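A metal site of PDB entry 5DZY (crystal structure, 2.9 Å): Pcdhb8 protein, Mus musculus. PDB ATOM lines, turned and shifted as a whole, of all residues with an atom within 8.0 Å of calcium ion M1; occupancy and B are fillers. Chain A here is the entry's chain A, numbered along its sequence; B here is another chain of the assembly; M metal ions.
The side-chain carboxylate (OD2) of Asp 240 is bound to calcium ion M1, 2.1 Å away. OD1 of Asn 208 binds calcium ion M1 (2.4 Å). O of Asn 210 is bound to calcium ion M1. O of His 246 binds calcium ion M1, 2.6 Å away. The side-chain carboxylate (OD2) of Asp 294 binds calcium ion M1 (2.9 Å). Calcium ion M1 has five donor atoms within binding distance. Slightly farther from calcium ion M1 lies OD1 of Asp 240 (2.9 Å). Slightly farther from calcium ion M1 lies OD2 of Asp 242 (3.0 Å).
OD1 of Asp 240 sits at hydrogen-bond distance from N of Asp 242. The side-chain amide oxygen (OD1) of Asn 208 lies close to the side-chain carboxylate (OD2) of Asp 242, at 2.8 Å. The side-chain amide oxygen of Gln 115 of chain B lies close to the side-chain amide nitrogen of Asn 208 (3.3 Å). The side-chain carboxylate (OD2) of Asp 242 is in hydrogen-bond range of the backbone NH (N) of Asn 210. OD1 of Asp 209 lies close to ND2 of Asn 210, 2.8 Å away. OD1 of Asp 294 is in hydrogen-bond range of N of Leu 298 (3.0 Å). The backbone NH of Gly 296 is in hydrogen-bond range of the side-chain carboxylate of Asp 294 (2.9 Å). The backbone NH (N) of Gly 297 is in hydrogen-bond range of the side-chain carboxylate (OD1) of Asp 294.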
ATOM      1  N   GLU A 175      -9.626 -16.150  20.412  1.00  0.00           N
ATOM      2  CA  GLU A 175      -8.542 -15.716  21.273  1.00  0.00           C
ATOM      3  C   GLU A 175      -8.075 -16.853  22.182  1.00  0.00           C
ATOM      4  O   GLU A 175      -6.979 -16.814  22.732  1.00  0.00           O
ATOM      5  CB  GLU A 175      -8.963 -14.511  22.111  1.00  0.00           C
ATOM      6  CG  GLU A 175      -9.083 -13.211  21.314  1.00  0.00           C
ATOM      7  CD  GLU A 175     -10.257 -13.209  20.350  1.00  0.00           C
ATOM      8  OE1 GLU A 175     -11.276 -13.858  20.653  1.00  0.00           O
ATOM      9  OE2 GLU A 175     -10.151 -12.574  19.278  1.00  0.00           O
ATOM     10  N   ASP A 206     -12.744 -14.590  13.038  1.00  0.00           N
ATOM     11  CA  ASP A 206     -12.514 -13.545  14.041  1.00  0.00           C
ATOM     12  C   ASP A 206     -13.666 -12.541  14.115  1.00  0.00           C
ATOM     13  O   ASP A 206     -14.141 -12.054  13.093  1.00  0.00           O
ATOM     14  CB  ASP A 206     -11.213 -12.799  13.738  1.00  0.00           C
ATOM     15  CG  ASP A 206     -10.920 -11.707  14.742  1.00  0.00           C
ATOM     16  OD1 ASP A 206     -11.290 -11.865  15.923  1.00  0.00           O
ATOM     17  OD2 ASP A 206     -10.310 -10.679  14.354  1.00  0.00           O
ATOM     18  N   ILE A 207     -14.080 -12.232  15.341  1.00  0.00           N
ATOM     19  CA  ILE A 207     -15.070 -11.182  15.568  1.00  0.00           C
ATOM     20  C   ILE A 207     -14.504 -10.151  16.537  1.00  0.00           C
ATOM     21  O   ILE A 207     -13.899 -10.507  17.544  1.00  0.00           O
ATOM     22  CB  ILE A 207     -16.396 -11.759  16.129  1.00  0.00           C
ATOM     23  CG1 ILE A 207     -16.976 -12.807  15.180  1.00  0.00           C
ATOM     24  CG2 ILE A 207     -17.410 -10.647  16.346  1.00  0.00           C
ATOM     25  CD1 ILE A 207     -17.358 -12.256  13.825  1.00  0.00           C
ATOM     26  N   ASN A 208     -14.684  -8.868  16.210  1.00  0.00           N
ATOM     27  CA  ASN A 208     -14.181  -7.787  17.050  1.00  0.00           C
ATOM     28  C   ASN A 208     -14.969  -7.690  18.345  1.00  0.00           C
ATOM     29  O   ASN A 208     -15.909  -6.890  18.452  1.00  0.00           O
ATOM     30  CB  ASN A 208     -14.214  -6.460  16.295  1.00  0.00           C
ATOM     31  CG  ASN A 208     -13.591  -5.307  17.084  1.00  0.00           C
ATOM     32  OD1 ASN A 208     -12.931  -5.521  18.104  1.00  0.00           O
ATOM     33  ND2 ASN A 208     -13.796  -4.089  16.610  1.00  0.00           N
ATOM     34  N   ASP A 209     -14.611  -8.514  19.318  1.00  0.00           N
ATOM     35  CA  ASP A 209     -15.270  -8.513  20.619  1.00  0.00           C
ATOM     36  C   ASP A 209     -14.305  -8.027  21.703  1.00  0.00           C
ATOM     37  O   ASP A 209     -14.637  -7.991  22.880  1.00  0.00           O
ATOM     38  CB  ASP A 209     -15.810  -9.909  20.953  1.00  0.00           C
ATOM     39  CG  ASP A 209     -14.728 -10.975  20.918  1.00  0.00           C
ATOM     40  OD1 ASP A 209     -13.633 -10.716  20.377  1.00  0.00           O
ATOM     41  OD2 ASP A 209     -14.981 -12.091  21.438  1.00  0.00           O
ATOM     42  N   ASN A 210     -13.102  -7.643  21.276  1.00  0.00           N
ATOM     43  CA  ASN A 210     -12.099  -7.110  22.185  1.00  0.00           C
ATOM     44  C   ASN A 210     -11.786  -5.642  21.900  1.00  0.00           C
ATOM     45  O   ASN A 210     -11.607  -5.246  20.752  1.00  0.00           O
ATOM     46  CB  ASN A 210     -10.811  -7.935  22.115  1.00  0.00           C
ATOM     47  CG  ASN A 210     -10.961  -9.299  22.752  1.00  0.00           C
ATOM     48  OD1 ASN A 210     -10.757  -9.449  23.958  1.00  0.00           O
ATOM     49  ND2 ASN A 210     -11.318 -10.293  21.950  1.00  0.00           N
ATOM     50  N   ALA A 211     -11.712  -4.853  22.961  1.00  0.00           N
ATOM     51  CA  ALA A 211     -11.406  -3.425  22.854  1.00  0.00           C
ATOM     52  C   ALA A 211      -9.913  -3.172  23.042  1.00  0.00           C
ATOM     53  O   ALA A 211      -9.284  -3.821  23.884  1.00  0.00           O
ATOM     54  CB  ALA A 211     -12.215  -2.634  23.878  1.00  0.00           C
ATOM     55  N   PRO A 212      -9.359  -2.239  22.274  1.00  0.00           N
ATOM     56  CA  PRO A 212      -7.931  -1.902  22.360  1.00  0.00           C
ATOM     57  C   PRO A 212      -7.545  -1.303  23.704  1.00  0.00           C
ATOM     58  O   PRO A 212      -8.298  -0.513  24.274  1.00  0.00           O
ATOM     59  CB  PRO A 212      -7.741  -0.874  21.236  1.00  0.00           C
ATOM     60  CG  PRO A 212      -9.099  -0.297  21.008  1.00  0.00           C
ATOM     61  CD  PRO A 212     -10.048  -1.430  21.250  1.00  0.00           C
ATOM     62  N   GLN A 213      -6.375  -1.679  24.211  1.00  0.00           N
ATOM     63  CA  GLN A 213      -5.879  -1.157  25.473  1.00  0.00           C
ATOM     64  C   GLN A 213      -4.466  -0.608  25.318  1.00  0.00           C
ATOM     65  O   GLN A 213      -3.661  -1.150  24.559  1.00  0.00           O
ATOM     66  CB  GLN A 213      -5.900  -2.246  26.561  1.00  0.00           C
ATOM     67  CG  GLN A 213      -7.273  -2.791  26.876  1.00  0.00           C
ATOM     68  CD  GLN A 213      -7.245  -3.810  27.992  1.00  0.00           C
ATOM     69  OE1 GLN A 213      -6.253  -3.936  28.706  1.00  0.00           O
ATOM     70  NE2 GLN A 213      -8.340  -4.552  28.151  1.00  0.00           N
ATOM     71  N   ARG A 239      -2.535  -1.996  22.044  1.00  0.00           N
ATOM     72  CA  ARG A 239      -2.603  -3.344  21.480  1.00  0.00           C
ATOM     73  C   ARG A 239      -4.015  -3.904  21.503  1.00  0.00           C
ATOM     74  O   ARG A 239      -4.782  -3.680  22.437  1.00  0.00           O
ATOM     75  CB  ARG A 239      -1.661  -4.280  22.238  1.00  0.00           C
ATOM     76  CG  ARG A 239      -0.187  -3.969  22.035  1.00  0.00           C
ATOM     77  CD  ARG A 239       0.177  -4.035  20.558  1.00  0.00           C
ATOM     78  NE  ARG A 239       1.566  -3.656  20.321  1.00  0.00           N
ATOM     79  CZ  ARG A 239       1.971  -2.407  20.090  1.00  0.00           C
ATOM     80  NH1 ARG A 239       3.253  -2.155  19.875  1.00  0.00           N
ATOM     81  NH2 ARG A 239       1.089  -1.423  20.056  1.00  0.00           N
ATOM     82  N   ASP A 240      -4.359  -4.641  20.449  1.00  0.00           N
ATOM     83  CA  ASP A 240      -5.670  -5.272  20.327  1.00  0.00           C
ATOM     84  C   ASP A 240      -5.525  -6.786  20.330  1.00  0.00           C
ATOM     85  O   ASP A 240      -4.609  -7.341  19.724  1.00  0.00           O
ATOM     86  CB  ASP A 240      -6.362  -4.802  19.046  1.00  0.00           C
ATOM     87  CG  ASP A 240      -7.857  -5.091  19.048  1.00  0.00           C
ATOM     88  OD1 ASP A 240      -8.311  -5.908  19.873  1.00  0.00           O
ATOM     89  OD2 ASP A 240      -8.571  -4.508  18.204  1.00  0.00           O
ATOM     90  N   LEU A 241      -6.442  -7.468  21.021  1.00  0.00           N
ATOM     91  CA  LEU A 241      -6.404  -8.914  21.124  1.00  0.00           C
ATOM     92  C   LEU A 241      -6.921  -9.585  19.858  1.00  0.00           C
ATOM     93  O   LEU A 241      -6.597 -10.740  19.578  1.00  0.00           O
ATOM     94  CB  LEU A 241      -7.203  -9.390  22.330  1.00  0.00           C
ATOM     95  CG  LEU A 241      -6.661  -8.951  23.699  1.00  0.00           C
ATOM     96  CD1 LEU A 241      -7.516  -9.518  24.825  1.00  0.00           C
ATOM     97  CD2 LEU A 241      -5.212  -9.368  23.857  1.00  0.00           C
ATOM     98  N   ASP A 242      -7.709  -8.857  19.081  1.00  0.00           N
ATOM     99  CA  ASP A 242      -8.237  -9.375  17.819  1.00  0.00           C
ATOM    100  C   ASP A 242      -7.178  -9.304  16.722  1.00  0.00           C
ATOM    101  O   ASP A 242      -6.092  -8.769  16.929  1.00  0.00           O
ATOM    102  CB  ASP A 242      -9.490  -8.598  17.398  1.00  0.00           C
ATOM    103  CG  ASP A 242     -10.655  -8.805  18.352  1.00  0.00           C
ATOM    104  OD1 ASP A 242     -10.740  -9.904  18.940  1.00  0.00           O
ATOM    105  OD2 ASP A 242     -11.477  -7.874  18.505  1.00  0.00           O
ATOM    106  N   ALA A 243      -7.510  -9.840  15.550  1.00  0.00           N
ATOM    107  CA  ALA A 243      -6.583  -9.853  14.433  1.00  0.00           C
ATOM    108  C   ALA A 243      -7.194  -9.241  13.180  1.00  0.00           C
ATOM    109  O   ALA A 243      -8.408  -9.079  13.093  1.00  0.00           O
ATOM    110  CB  ALA A 243      -6.122 -11.283  14.144  1.00  0.00           C
ATOM    111  N   GLY A 244      -6.349  -8.904  12.215  1.00  0.00           N
ATOM    112  CA  GLY A 244      -6.802  -8.323  10.965  1.00  0.00           C
ATOM    113  C   GLY A 244      -7.266  -6.887  11.109  1.00  0.00           C
ATOM    114  O   GLY A 244      -6.694  -6.116  11.888  1.00  0.00           O
ATOM    115  N   ILE A 245      -8.305  -6.531  10.356  1.00  0.00           N
ATOM    116  CA  ILE A 245      -8.869  -5.187  10.410  1.00  0.00           C
ATOM    117  C   ILE A 245      -9.525  -4.936  11.767  1.00  0.00           C
ATOM    118  O   ILE A 245      -9.563  -3.805  12.254  1.00  0.00           O
ATOM    119  CB  ILE A 245      -9.906  -4.973   9.293  1.00  0.00           C
ATOM    120  CG1 ILE A 245      -9.321  -5.391   7.939  1.00  0.00           C
ATOM    121  CG2 ILE A 245     -10.369  -3.519   9.239  1.00  0.00           C
ATOM    122  CD1 ILE A 245      -8.083  -4.607   7.536  1.00  0.00           C
ATOM    123  N   HIS A 246     -10.019  -6.000  12.388  1.00  0.00           N
ATOM    124  CA  HIS A 246     -10.668  -5.904  13.695  1.00  0.00           C
ATOM    125  C   HIS A 246      -9.654  -5.604  14.792  1.00  0.00           C
ATOM    126  O   HIS A 246     -10.024  -5.316  15.925  1.00  0.00           O
ATOM    127  CB  HIS A 246     -11.412  -7.203  14.012  1.00  0.00           C
ATOM    128  CG  HIS A 246     -12.451  -7.567  12.997  1.00  0.00           C
ATOM    129  ND1 HIS A 246     -13.799  -7.377  13.219  1.00  0.00           N
ATOM    130  CD2 HIS A 246     -12.351  -8.109  11.765  1.00  0.00           C
ATOM    131  CE1 HIS A 246     -14.484  -7.788  12.161  1.00  0.00           C
ATOM    132  NE2 HIS A 246     -13.620  -8.245  11.261  1.00  0.00           N
ATOM    133  N   GLY A 247      -8.366  -5.671  14.451  1.00  0.00           N
ATOM    134  CA  GLY A 247      -7.310  -5.430  15.416  1.00  0.00           C
ATOM    135  C   GLY A 247      -6.565  -4.131  15.201  1.00  0.00           C
ATOM    136  O   GLY A 247      -5.849  -3.664  16.092  1.00  0.00           O
ATOM    137  N   ASN A 248      -6.723  -3.539  14.022  1.00  0.00           N
ATOM    138  CA  ASN A 248      -6.088  -2.255  13.721  1.00  0.00           C
ATOM    139  C   ASN A 248      -6.636  -1.133  14.584  1.00  0.00           C
ATOM    140  O   ASN A 248      -7.846  -1.035  14.776  1.00  0.00           O
ATOM    141  CB  ASN A 248      -6.255  -1.906  12.238  1.00  0.00           C
ATOM    142  CG  ASN A 248      -5.334  -2.720  11.340  1.00  0.00           C
ATOM    143  OD1 ASN A 248      -4.244  -3.125  11.755  1.00  0.00           O
ATOM    144  ND2 ASN A 248      -5.771  -2.957  10.110  1.00  0.00           N
ATOM    145  N   VAL A 249      -5.750  -0.290  15.101  1.00  0.00           N
ATOM    146  CA  VAL A 249      -6.152   0.805  15.962  1.00  0.00           C
ATOM    147  C   VAL A 249      -5.932   2.165  15.313  1.00  0.00           C
ATOM    148  O   VAL A 249      -5.106   2.302  14.412  1.00  0.00           O
ATOM    149  CB  VAL A 249      -5.392   0.769  17.307  1.00  0.00           C
ATOM    150  CG1 VAL A 249      -5.804  -0.450  18.116  1.00  0.00           C
ATOM    151  CG2 VAL A 249      -3.894   0.797  17.069  1.00  0.00           C
ATOM    152  N   THR A 293      -9.025   3.691  18.828  1.00  0.00           N
ATOM    153  CA  THR A 293     -10.283   3.067  18.440  1.00  0.00           C
ATOM    154  C   THR A 293     -10.106   2.178  17.207  1.00  0.00           C
ATOM    155  O   THR A 293      -9.473   2.576  16.236  1.00  0.00           O
ATOM    156  CB  THR A 293     -11.366   4.122  18.138  1.00  0.00           C
ATOM    157  OG1 THR A 293     -11.476   5.021  19.251  1.00  0.00           O
ATOM    158  CG2 THR A 293     -12.709   3.467  17.877  1.00  0.00           C
ATOM    159  N   ASP A 294     -10.661   0.966  17.263  1.00  0.00           N
ATOM    160  CA  ASP A 294     -10.563   0.040  16.142  1.00  0.00           C
ATOM    161  C   ASP A 294     -11.547   0.399  15.028  1.00  0.00           C
ATOM    162  O   ASP A 294     -12.077   1.507  14.985  1.00  0.00           O
ATOM    163  CB  ASP A 294     -10.808  -1.405  16.610  1.00  0.00           C
ATOM    164  CG  ASP A 294     -12.081  -1.549  17.422  1.00  0.00           C
ATOM    165  OD1 ASP A 294     -13.003  -0.714  17.287  1.00  0.00           O
ATOM    166  OD2 ASP A 294     -12.168  -2.514  18.210  1.00  0.00           O
ATOM    167  N   SER A 295     -11.781  -0.544  14.120  1.00  0.00           N
ATOM    168  CA  SER A 295     -12.716  -0.341  13.023  1.00  0.00           C
ATOM    169  C   SER A 295     -14.134  -0.681  13.435  1.00  0.00           C
ATOM    170  O   SER A 295     -15.071  -0.621  12.628  1.00  0.00           O
ATOM    171  CB  SER A 295     -12.305  -1.164  11.801  1.00  0.00           C
ATOM    172  OG  SER A 295     -12.376  -2.555  12.091  1.00  0.00           O
ATOM    173  N   GLY A 296     -14.305  -1.044  14.710  1.00  0.00           N
ATOM    174  CA  GLY A 296     -15.596  -1.453  15.223  1.00  0.00           C
ATOM    175  C   GLY A 296     -16.250  -0.417  16.114  1.00  0.00           C
ATOM    176  O   GLY A 296     -17.466  -0.346  16.216  1.00  0.00           O
ATOM    177  N   GLY A 297     -15.420   0.391  16.782  1.00  0.00           N
ATOM    178  CA  GLY A 297     -15.935   1.408  17.678  1.00  0.00           C
ATOM    179  C   GLY A 297     -15.454   1.221  19.100  1.00  0.00           C
ATOM    180  O   GLY A 297     -15.504   2.143  19.907  1.00  0.00           O
ATOM    181  N   LEU A 298     -15.007   0.010  19.409  1.00  0.00           N
ATOM    182  CA  LEU A 298     -14.437  -0.288  20.706  1.00  0.00           C
ATOM    183  C   LEU A 298     -13.206   0.587  20.919  1.00  0.00           C
ATOM    184  O   LEU A 298     -12.351   0.699  20.044  1.00  0.00           O
ATOM    185  CB  LEU A 298     -14.080  -1.765  20.818  1.00  0.00           C
ATOM    186  CG  LEU A 298     -15.255  -2.733  20.681  1.00  0.00           C
ATOM    187  CD1 LEU A 298     -14.795  -4.173  20.857  1.00  0.00           C
ATOM    188  CD2 LEU A 298     -16.352  -2.385  21.674  1.00  0.00           C
ATOM    189  N   SER A 299     -13.119   1.211  22.084  1.00  0.00           N
ATOM    190  CA  SER A 299     -12.066   2.190  22.334  1.00  0.00           C
ATOM    191  C   SER A 299     -11.317   1.955  23.637  1.00  0.00           C
ATOM    192  O   SER A 299     -11.789   1.272  24.540  1.00  0.00           O
ATOM    193  CB  SER A 299     -12.651   3.607  22.325  1.00  0.00           C
ATOM    194  OG  SER A 299     -13.661   3.738  23.316  1.00  0.00           O
ATOM    195  N   GLN B 115     -20.260  -0.587  16.061  1.00  0.00           N
ATOM    196  CA  GLN B 115     -20.741  -1.891  15.616  1.00  0.00           C
ATOM    197  C   GLN B 115     -22.236  -2.085  15.857  1.00  0.00           C
ATOM    198  O   GLN B 115     -22.820  -1.464  16.754  1.00  0.00           O
ATOM    199  CB  GLN B 115     -19.974  -3.008  16.312  1.00  0.00           C
ATOM    200  CG  GLN B 115     -18.607  -3.282  15.714  1.00  0.00           C
ATOM    201  CD  GLN B 115     -17.810  -4.282  16.511  1.00  0.00           C
ATOM    202  OE1 GLN B 115     -16.885  -4.909  15.996  1.00  0.00           O
ATOM    203  NE2 GLN B 115     -18.149  -4.430  17.790  1.00  0.00           N
HETATM  204 CA    CA M   1     -10.652  -4.951  18.403  1.00  0.00          CA
HETATM  205 CA    CA M   2     -12.253 -11.879  18.724  1.00  0.00          CA
